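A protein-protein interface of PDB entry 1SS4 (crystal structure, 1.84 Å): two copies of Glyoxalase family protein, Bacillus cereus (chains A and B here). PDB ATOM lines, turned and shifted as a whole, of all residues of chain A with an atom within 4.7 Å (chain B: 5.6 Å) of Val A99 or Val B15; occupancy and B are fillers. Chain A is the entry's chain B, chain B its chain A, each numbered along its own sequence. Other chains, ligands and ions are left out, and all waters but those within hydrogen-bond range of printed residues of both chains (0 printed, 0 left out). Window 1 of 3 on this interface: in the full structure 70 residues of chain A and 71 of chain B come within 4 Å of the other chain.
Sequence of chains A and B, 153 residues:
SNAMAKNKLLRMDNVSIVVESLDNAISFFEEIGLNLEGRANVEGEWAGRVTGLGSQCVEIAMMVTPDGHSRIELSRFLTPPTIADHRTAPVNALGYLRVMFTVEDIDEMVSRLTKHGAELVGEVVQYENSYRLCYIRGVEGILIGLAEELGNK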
ATOM      1  N   MET A  12      32.338   6.702  15.080  1.00  0.00           N
ATOM      2  CA  MET A  12      31.397   6.744  16.198  1.00  0.00           C
ATOM      3  C   MET A  12      32.201   6.056  17.290  1.00  0.00           C
ATOM      4  O   MET A  12      32.297   4.819  17.320  1.00  0.00           O
ATOM      5  CB  MET A  12      30.124   5.955  15.867  1.00  0.00           C
ATOM      6  CG  MET A  12      29.034   6.017  16.932  1.00  0.00           C
ATOM      7  SD  MET A  12      27.338   5.267  16.265  1.00  0.00           S
ATOM      8  CE  MET A  12      27.384   3.563  17.227  1.00  0.00           C
ATOM      9  N   VAL A  15      29.066   4.555  22.753  1.00  0.00           N
ATOM     10  CA  VAL A  15      27.729   4.900  23.213  1.00  0.00           C
ATOM     11  C   VAL A  15      27.898   4.800  24.716  1.00  0.00           C
ATOM     12  O   VAL A  15      28.431   3.802  25.200  1.00  0.00           O
ATOM     13  CB  VAL A  15      26.652   3.870  22.751  1.00  0.00           C
ATOM     14  CG1 VAL A  15      25.311   4.221  23.375  1.00  0.00           C
ATOM     15  CG2 VAL A  15      26.518   3.904  21.230  1.00  0.00           C
ATOM     16  N   ILE A  72      31.455   0.739  24.412  1.00  0.00           N
ATOM     17  CA  ILE A  72      30.386   1.144  25.307  1.00  0.00           C
ATOM     18  C   ILE A  72      31.066   1.745  26.508  1.00  0.00           C
ATOM     19  O   ILE A  72      31.923   1.122  27.116  1.00  0.00           O
ATOM     20  CB  ILE A  72      29.536  -0.036  25.774  1.00  0.00           C
ATOM     21  CG1 ILE A  72      28.737  -0.574  24.593  1.00  0.00           C
ATOM     22  CG2 ILE A  72      28.631   0.381  26.940  1.00  0.00           C
ATOM     23  CD1 ILE A  72      27.891  -1.739  24.968  1.00  0.00           C
ATOM     24  N   TYR A  96      16.980   7.323  23.180  1.00  0.00           N
ATOM     25  CA  TYR A  96      17.845   6.159  22.937  1.00  0.00           C
ATOM     26  C   TYR A  96      17.081   4.909  23.365  1.00  0.00           C
ATOM     27  O   TYR A  96      16.481   4.889  24.442  1.00  0.00           O
ATOM     28  CB  TYR A  96      19.145   6.289  23.736  1.00  0.00           C
ATOM     29  CG  TYR A  96      20.105   7.305  23.137  1.00  0.00           C
ATOM     30  CD1 TYR A  96      20.777   7.020  21.950  1.00  0.00           C
ATOM     31  CD2 TYR A  96      20.351   8.538  23.769  1.00  0.00           C
ATOM     32  CE1 TYR A  96      21.664   7.922  21.392  1.00  0.00           C
ATOM     33  CE2 TYR A  96      21.246   9.452  23.229  1.00  0.00           C
ATOM     34  CZ  TYR A  96      21.899   9.133  22.031  1.00  0.00           C
ATOM     35  OH  TYR A  96      22.801   9.987  21.448  1.00  0.00           O
ATOM     36  N   ARG A  98      18.168   1.083  22.392  1.00  0.00           N
ATOM     37  CA  ARG A  98      19.014  -0.046  22.726  1.00  0.00           C
ATOM     38  C   ARG A  98      20.175  -0.185  21.775  1.00  0.00           C
ATOM     39  O   ARG A  98      20.145   0.339  20.654  1.00  0.00           O
ATOM     40  CB  ARG A  98      18.180  -1.336  22.633  1.00  0.00           C
ATOM     41  CG  ARG A  98      17.485  -1.441  21.235  1.00  0.00           C
ATOM     42  CD  ARG A  98      17.989  -2.609  20.435  1.00  0.00           C
ATOM     43  NE  ARG A  98      17.614  -2.570  19.013  1.00  0.00           N
ATOM     44  CZ  ARG A  98      18.311  -1.947  18.058  1.00  0.00           C
ATOM     45  NH1 ARG A  98      19.423  -1.284  18.355  1.00  0.00           N
ATOM     46  NH2 ARG A  98      17.939  -2.049  16.785  1.00  0.00           N
ATOM     47  N   VAL A  99      21.210  -0.875  22.238  1.00  0.00           N
ATOM     48  CA  VAL A  99      22.323  -1.188  21.380  1.00  0.00           C
ATOM     49  C   VAL A  99      22.047  -2.640  20.948  1.00  0.00           C
ATOM     50  O   VAL A  99      21.528  -3.470  21.734  1.00  0.00           O
ATOM     51  CB  VAL A  99      23.710  -1.083  22.086  1.00  0.00           C
ATOM     52  CG1 VAL A  99      24.057   0.398  22.301  1.00  0.00           C
ATOM     53  CG2 VAL A  99      23.708  -1.845  23.412  1.00  0.00           C
ATOM     54  N   MET A 100      22.390  -2.928  19.702  1.00  0.00           N
ATOM     55  CA  MET A 100      22.191  -4.256  19.129  1.00  0.00           C
ATOM     56  C   MET A 100      23.511  -4.970  18.836  1.00  0.00           C
ATOM     57  O   MET A 100      24.402  -4.404  18.215  1.00  0.00           O
ATOM     58  CB  MET A 100      21.364  -4.129  17.845  1.00  0.00           C
ATOM     59  CG  MET A 100      21.399  -5.358  16.972  1.00  0.00           C
ATOM     60  SD  MET A 100      20.161  -6.689  17.571  1.00  0.00           S
ATOM     61  CE  MET A 100      18.646  -5.888  16.694  1.00  0.00           C
ATOM     62  N   PHE A 101      23.627  -6.222  19.289  1.00  0.00           N
ATOM     63  CA  PHE A 101      24.839  -7.020  19.066  1.00  0.00           C
ATOM     64  C   PHE A 101      24.544  -8.263  18.210  1.00  0.00           C
ATOM     65  O   PHE A 101      23.502  -8.888  18.359  1.00  0.00           O
ATOM     66  CB  PHE A 101      25.419  -7.518  20.382  1.00  0.00           C
ATOM     67  CG  PHE A 101      25.820  -6.443  21.318  1.00  0.00           C
ATOM     68  CD1 PHE A 101      27.022  -5.770  21.147  1.00  0.00           C
ATOM     69  CD2 PHE A 101      24.998  -6.112  22.397  1.00  0.00           C
ATOM     70  CE1 PHE A 101      27.416  -4.775  22.057  1.00  0.00           C
ATOM     71  CE2 PHE A 101      25.383  -5.116  23.308  1.00  0.00           C
ATOM     72  CZ  PHE A 101      26.593  -4.454  23.132  1.00  0.00           C
ATOM     73  N   LEU A 143      17.847  -2.244  28.297  1.00  0.00           N
ATOM     74  CA  LEU A 143      17.431  -2.921  27.069  1.00  0.00           C
ATOM     75  C   LEU A 143      18.586  -3.146  26.111  1.00  0.00           C
ATOM     76  O   LEU A 143      19.337  -2.214  25.812  1.00  0.00           O
ATOM     77  CB  LEU A 143      16.356  -2.077  26.366  1.00  0.00           C
ATOM     78  CG  LEU A 143      15.674  -2.670  25.126  1.00  0.00           C
ATOM     79  CD1 LEU A 143      14.962  -3.954  25.537  1.00  0.00           C
ATOM     80  CD2 LEU A 143      14.666  -1.673  24.533  1.00  0.00           C
ATOM     81  N   ILE A 144      18.709  -4.376  25.617  1.00  0.00           N
ATOM     82  CA  ILE A 144      19.770  -4.723  24.681  1.00  0.00           C
ATOM     83  C   ILE A 144      19.181  -5.631  23.601  1.00  0.00           C
ATOM     84  O   ILE A 144      18.251  -6.401  23.874  1.00  0.00           O
ATOM     85  CB  ILE A 144      20.937  -5.426  25.446  1.00  0.00           C
ATOM     86  CG1 ILE A 144      21.789  -4.349  26.143  1.00  0.00           C
ATOM     87  CG2 ILE A 144      21.778  -6.278  24.521  1.00  0.00           C
ATOM     88  CD1 ILE A 144      22.879  -4.899  26.979  1.00  0.00           C
ATOM     89  N   GLY A 145      19.691  -5.508  22.376  1.00  0.00           N
ATOM     90  CA  GLY A 145      19.215  -6.348  21.290  1.00  0.00           C
ATOM     91  C   GLY A 145      20.282  -7.370  20.955  1.00  0.00           C
ATOM     92  O   GLY A 145      21.481  -7.126  21.157  1.00  0.00           O
ATOM     93  N   MET B  12      28.895  -4.872  17.161  1.00  0.00           N
ATOM     94  CA  MET B  12      27.776  -4.139  17.729  1.00  0.00           C
ATOM     95  C   MET B  12      27.167  -3.554  16.461  1.00  0.00           C
ATOM     96  O   MET B  12      27.727  -2.637  15.874  1.00  0.00           O
ATOM     97  CB  MET B  12      28.251  -3.022  18.656  1.00  0.00           C
ATOM     98  CG  MET B  12      27.092  -2.247  19.222  1.00  0.00           C
ATOM     99  SD  MET B  12      27.731  -0.958  20.523  1.00  0.00           S
ATOM    100  CE  MET B  12      28.108   0.486  19.290  1.00  0.00           C
ATOM    101  N   ASP B  13      26.046  -4.111  16.021  1.00  0.00           N
ATOM    102  CA  ASP B  13      25.405  -3.680  14.787  1.00  0.00           C
ATOM    103  C   ASP B  13      24.960  -2.230  14.730  1.00  0.00           C
ATOM    104  O   ASP B  13      25.183  -1.538  13.733  1.00  0.00           O
ATOM    105  CB  ASP B  13      24.204  -4.569  14.496  1.00  0.00           C
ATOM    106  CG  ASP B  13      23.818  -4.536  13.048  1.00  0.00           C
ATOM    107  OD1 ASP B  13      24.405  -5.324  12.259  1.00  0.00           O
ATOM    108  OD2 ASP B  13      22.949  -3.703  12.688  1.00  0.00           O
ATOM    109  N   ASN B  14      24.324  -1.760  15.791  1.00  0.00           N
ATOM    110  CA  ASN B  14      23.827  -0.394  15.799  1.00  0.00           C
ATOM    111  C   ASN B  14      23.259  -0.025  17.161  1.00  0.00           C
ATOM    112  O   ASN B  14      23.053  -0.889  18.019  1.00  0.00           O
ATOM    113  CB  ASN B  14      22.693  -0.249  14.766  1.00  0.00           C
ATOM    114  CG  ASN B  14      21.438  -1.094  15.136  1.00  0.00           C
ATOM    115  OD1 ASN B  14      20.696  -0.758  16.053  1.00  0.00           O
ATOM    116  ND2 ASN B  14      21.226  -2.194  14.418  1.00  0.00           N
ATOM    117  N   VAL B  15      23.030   1.268  17.342  1.00  0.00           N
ATOM    118  CA  VAL B  15      22.362   1.763  18.534  1.00  0.00           C
ATOM    119  C   VAL B  15      21.125   2.376  17.894  1.00  0.00           C
ATOM    120  O   VAL B  15      21.221   2.970  16.823  1.00  0.00           O
ATOM    121  CB  VAL B  15      23.160   2.854  19.262  1.00  0.00           C
ATOM    122  CG1 VAL B  15      23.550   3.942  18.288  1.00  0.00           C
ATOM    123  CG2 VAL B  15      22.313   3.438  20.383  1.00  0.00           C
ATOM    124  N   SER B  16      19.953   2.184  18.492  1.00  0.00           N
ATOM    125  CA  SER B  16      18.754   2.744  17.890  1.00  0.00           C
ATOM    126  C   SER B  16      18.166   3.811  18.756  1.00  0.00           C
ATOM    127  O   SER B  16      18.303   3.770  19.993  1.00  0.00           O
ATOM    128  CB  SER B  16      17.695   1.671  17.628  1.00  0.00           C
ATOM    129  OG  SER B  16      17.176   1.194  18.863  1.00  0.00           O
ATOM    130  N   ILE B  17      17.512   4.771  18.091  1.00  0.00           N
ATOM    131  CA  ILE B  17      16.875   5.906  18.761  1.00  0.00           C
ATOM    132  C   ILE B  17      15.433   5.994  18.229  1.00  0.00           C
ATOM    133  O   ILE B  17      15.214   5.890  17.022  1.00  0.00           O
ATOM    134  CB  ILE B  17      17.598   7.255  18.415  1.00  0.00           C
ATOM    135  CG1 ILE B  17      19.120   7.107  18.561  1.00  0.00           C
ATOM    136  CG2 ILE B  17      17.075   8.385  19.338  1.00  0.00           C
ATOM    137  CD1 ILE B  17      19.921   8.309  18.020  1.00  0.00           C
ATOM    138  N   ARG B  71      26.536   2.042  13.041  1.00  0.00           N
ATOM    139  CA  ARG B  71      25.227   2.397  12.542  1.00  0.00           C
ATOM    140  C   ARG B  71      24.297   2.929  13.618  1.00  0.00           C
ATOM    141  O   ARG B  71      24.384   2.537  14.785  1.00  0.00           O
ATOM    142  CB  ARG B  71      24.569   1.180  11.879  1.00  0.00           C
ATOM    143  CG  ARG B  71      25.199   0.754  10.562  1.00  0.00           C
ATOM    144  CD  ARG B  71      24.692  -0.627  10.113  1.00  0.00           C
ATOM    145  NE  ARG B  71      25.095  -0.880   8.735  1.00  0.00           N
ATOM    146  CZ  ARG B  71      26.314  -1.255   8.366  1.00  0.00           C
ATOM    147  NH1 ARG B  71      27.262  -1.445   9.277  1.00  0.00           N
ATOM    148  NH2 ARG B  71      26.596  -1.402   7.078  1.00  0.00           N
ATOM    149  N   ILE B  72      23.399   3.816  13.193  1.00  0.00           N
ATOM    150  CA  ILE B  72      22.381   4.383  14.064  1.00  0.00           C
ATOM    151  C   ILE B  72      21.047   4.050  13.404  1.00  0.00           C
ATOM    152  O   ILE B  72      20.789   4.419  12.255  1.00  0.00           O
ATOM    153  CB  ILE B  72      22.506   5.899  14.193  1.00  0.00           C
ATOM    154  CG1 ILE B  72      23.778   6.241  14.947  1.00  0.00           C
ATOM    155  CG2 ILE B  72      21.263   6.482  14.887  1.00  0.00           C
ATOM    156  CD1 ILE B  72      24.219   7.705  14.763  1.00  0.00           C
ATOM    157  N   GLU B  73      20.208   3.326  14.129  1.00  0.00           N
ATOM    158  CA  GLU B  73      18.895   2.968  13.614  1.00  0.00           C
ATOM    159  C   GLU B  73      17.900   3.956  14.187  1.00  0.00           C
ATOM    160  O   GLU B  73      17.808   4.115  15.409  1.00  0.00           O
ATOM    161  CB  GLU B  73      18.505   1.552  14.052  1.00  0.00           C
ATOM    162  CG  GLU B  73      17.192   1.072  13.447  1.00  0.00           C
ATOM    163  CD  GLU B  73      16.846  -0.373  13.832  1.00  0.00           C
ATOM    164  OE1 GLU B  73      17.706  -1.271  13.681  1.00  0.00           O
ATOM    165  OE2 GLU B  73      15.714  -0.619  14.281  1.00  0.00           O
ATOM    166  N   TYR B  96      20.800   4.969  28.922  1.00  0.00           N
ATOM    167  CA  TYR B  96      21.563   5.408  27.745  1.00  0.00           C
ATOM    168  C   TYR B  96      21.730   6.910  27.814  1.00  0.00           C
ATOM    169  O   TYR B  96      20.773   7.639  28.070  1.00  0.00           O
ATOM    170  CB  TYR B  96      20.840   5.009  26.460  1.00  0.00           C
ATOM    171  CG  TYR B  96      20.955   3.531  26.169  1.00  0.00           C
ATOM    172  CD1 TYR B  96      22.165   2.990  25.724  1.00  0.00           C
ATOM    173  CD2 TYR B  96      19.867   2.672  26.347  1.00  0.00           C
ATOM    174  CE1 TYR B  96      22.295   1.658  25.463  1.00  0.00           C
ATOM    175  CE2 TYR B  96      19.983   1.315  26.086  1.00  0.00           C
ATOM    176  CZ  TYR B  96      21.203   0.817  25.643  1.00  0.00           C
ATOM    177  OH  TYR B  96      21.361  -0.503  25.345  1.00  0.00           O
ATOM    178  N   VAL B  99      25.711   9.119  22.234  1.00  0.00           N
ATOM    179  CA  VAL B  99      26.680   8.500  21.351  1.00  0.00           C
ATOM    180  C   VAL B  99      27.692   9.637  21.107  1.00  0.00           C
ATOM    181  O   VAL B  99      27.312  10.811  21.018  1.00  0.00           O
ATOM    182  CB  VAL B  99      26.067   8.023  20.009  1.00  0.00           C
ATOM    183  CG1 VAL B  99      25.015   6.930  20.286  1.00  0.00           C
ATOM    184  CG2 VAL B  99      25.418   9.156  19.269  1.00  0.00           C
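Of the 11 printed residues of chain B, 10 touch a printed residue of chain A. Hydrophobic or aromatic side chains of chain B that line the printed part of chain A: Met B12, Val B15, Ile B17, Ile B72, Tyr B96 and Val B99. Hydrophobic or aromatic side chains of chain A within 4 Å of the printed part of chain B: Met A12, Val A15, Tyr A96, Val A99, Met A100, Phe A101 and Ile A144.
Of the printed residues of chain B, Val A99 touches Asn B14, Val B15 and Tyr B96. Of the printed residues of chain B, Arg A98 touches Asn B14, Val B15, Ser B16, Glu B73 and Tyr B96. Printed residues of chain A within 4 Å of Met B12: Met A12, Met A100 and Phe A101. Printed residues of chain A within 4 Å of Ser B16: Tyr A96 and Arg A98. The nearest printed residue of chain B that does not touch Val A99 is Met B12 (4.3 Å). The nearest printed residue of chain A that does not touch Val B15 is Val A15 (4.03 Å).
Among the printed residues, pairs that only touch across the chains: Met A12 with Met B12 (3.8 Å), Met A12 with Val B15 (3.996 Å), Met A12 with Ile B72 (3.9 Å), Val A15 with Val B99 (3.5 Å), Tyr A96 with Ser B16 (3.8 Å), Tyr A96 with Ile B17 (3.8 Å), Tyr A96 with Tyr B96 (3.5 Å), Arg A98 with Val B15 (3.4 Å), Arg A98 with Tyr B96 (3.5 Å), Val A99 with Asn B14 (3.5 Å), Val A99 with Val B15 (3.995 Å), Met A100 with Met B12 (3.4 Å), Phe A101 with Met B12 (3.8 Å) and Ile A144 with Tyr B96 (3.95 Å).
Met A12 touches Val B15, but with the chains exchanged Val A15 does not touch Met B12 (4.2 Å). Val A15 touches Val B99, and with the chains exchanged Val A99 touches Val B15. Tyr B96 touches its own counterpart, Tyr A96. Tyr A96 touches Val B99, and with the chains exchanged Val A99 touches Tyr B96. Positions printed for both chains: 12, 15, 72, 96 and 99. Of the 22 pairs that touch across the chains among the printed residues, 6 have their exchanged pair printed and touching as well.
The side-chain carboxylate (OD2) of Asp B13 sits at hydrogen-bond distance from the side-chain amide nitrogen (ND2) of Asn B14 (2.9 Å). The backbone NH (N) of Val B15 sits at hydrogen-bond distance from the backbone carbonyl oxygen (O) of Arg B71, at 3.2 Å. The backbone NH (N) of Glu B73 sits at hydrogen-bond distance from the backbone carbonyl oxygen (O) of Val B15, at 2.9 Å. N of Ile B17 sits at hydrogen-bond distance from O of Glu B73, at 2.8 Å. The backbone NH of Gly A145 sits at hydrogen-bond distance from the backbone carbonyl oxygen of Val A99 (2.8 Å). The backbone NH (N) of Phe A101 sits at hydrogen-bond distance from the backbone carbonyl oxygen (O) of Gly A145 (3.0 Å).
N of Asp B13 is in hydrogen-bond range of O of Met A100 (2.8 Å). NH1 of Arg A98 is in hydrogen-bond range of OD1 of Asn B14. The backbone NH of Met A100 lies within hydrogen-bond range of the backbone carbonyl oxygen of Asn B14 (2.7 Å). O of Arg A98 sits at hydrogen-bond distance from N of Ser B16. OE1 of Glu B73 lies within salt-bridge range of NH2 of Arg A98, at 3.2 Å. OH of Tyr B96 is in hydrogen-bond range of N of Val A99, 3.1 Å away. The backbone carbonyl oxygen of Leu A143 sits at hydrogen-bond distance from the side-chain hydroxyl of Tyr B96, 2.7 Å away. The backbone NH (N) of Val B99 lies within hydrogen-bond range of the side-chain hydroxyl (OH) of Tyr A96, at 3.1 Å.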
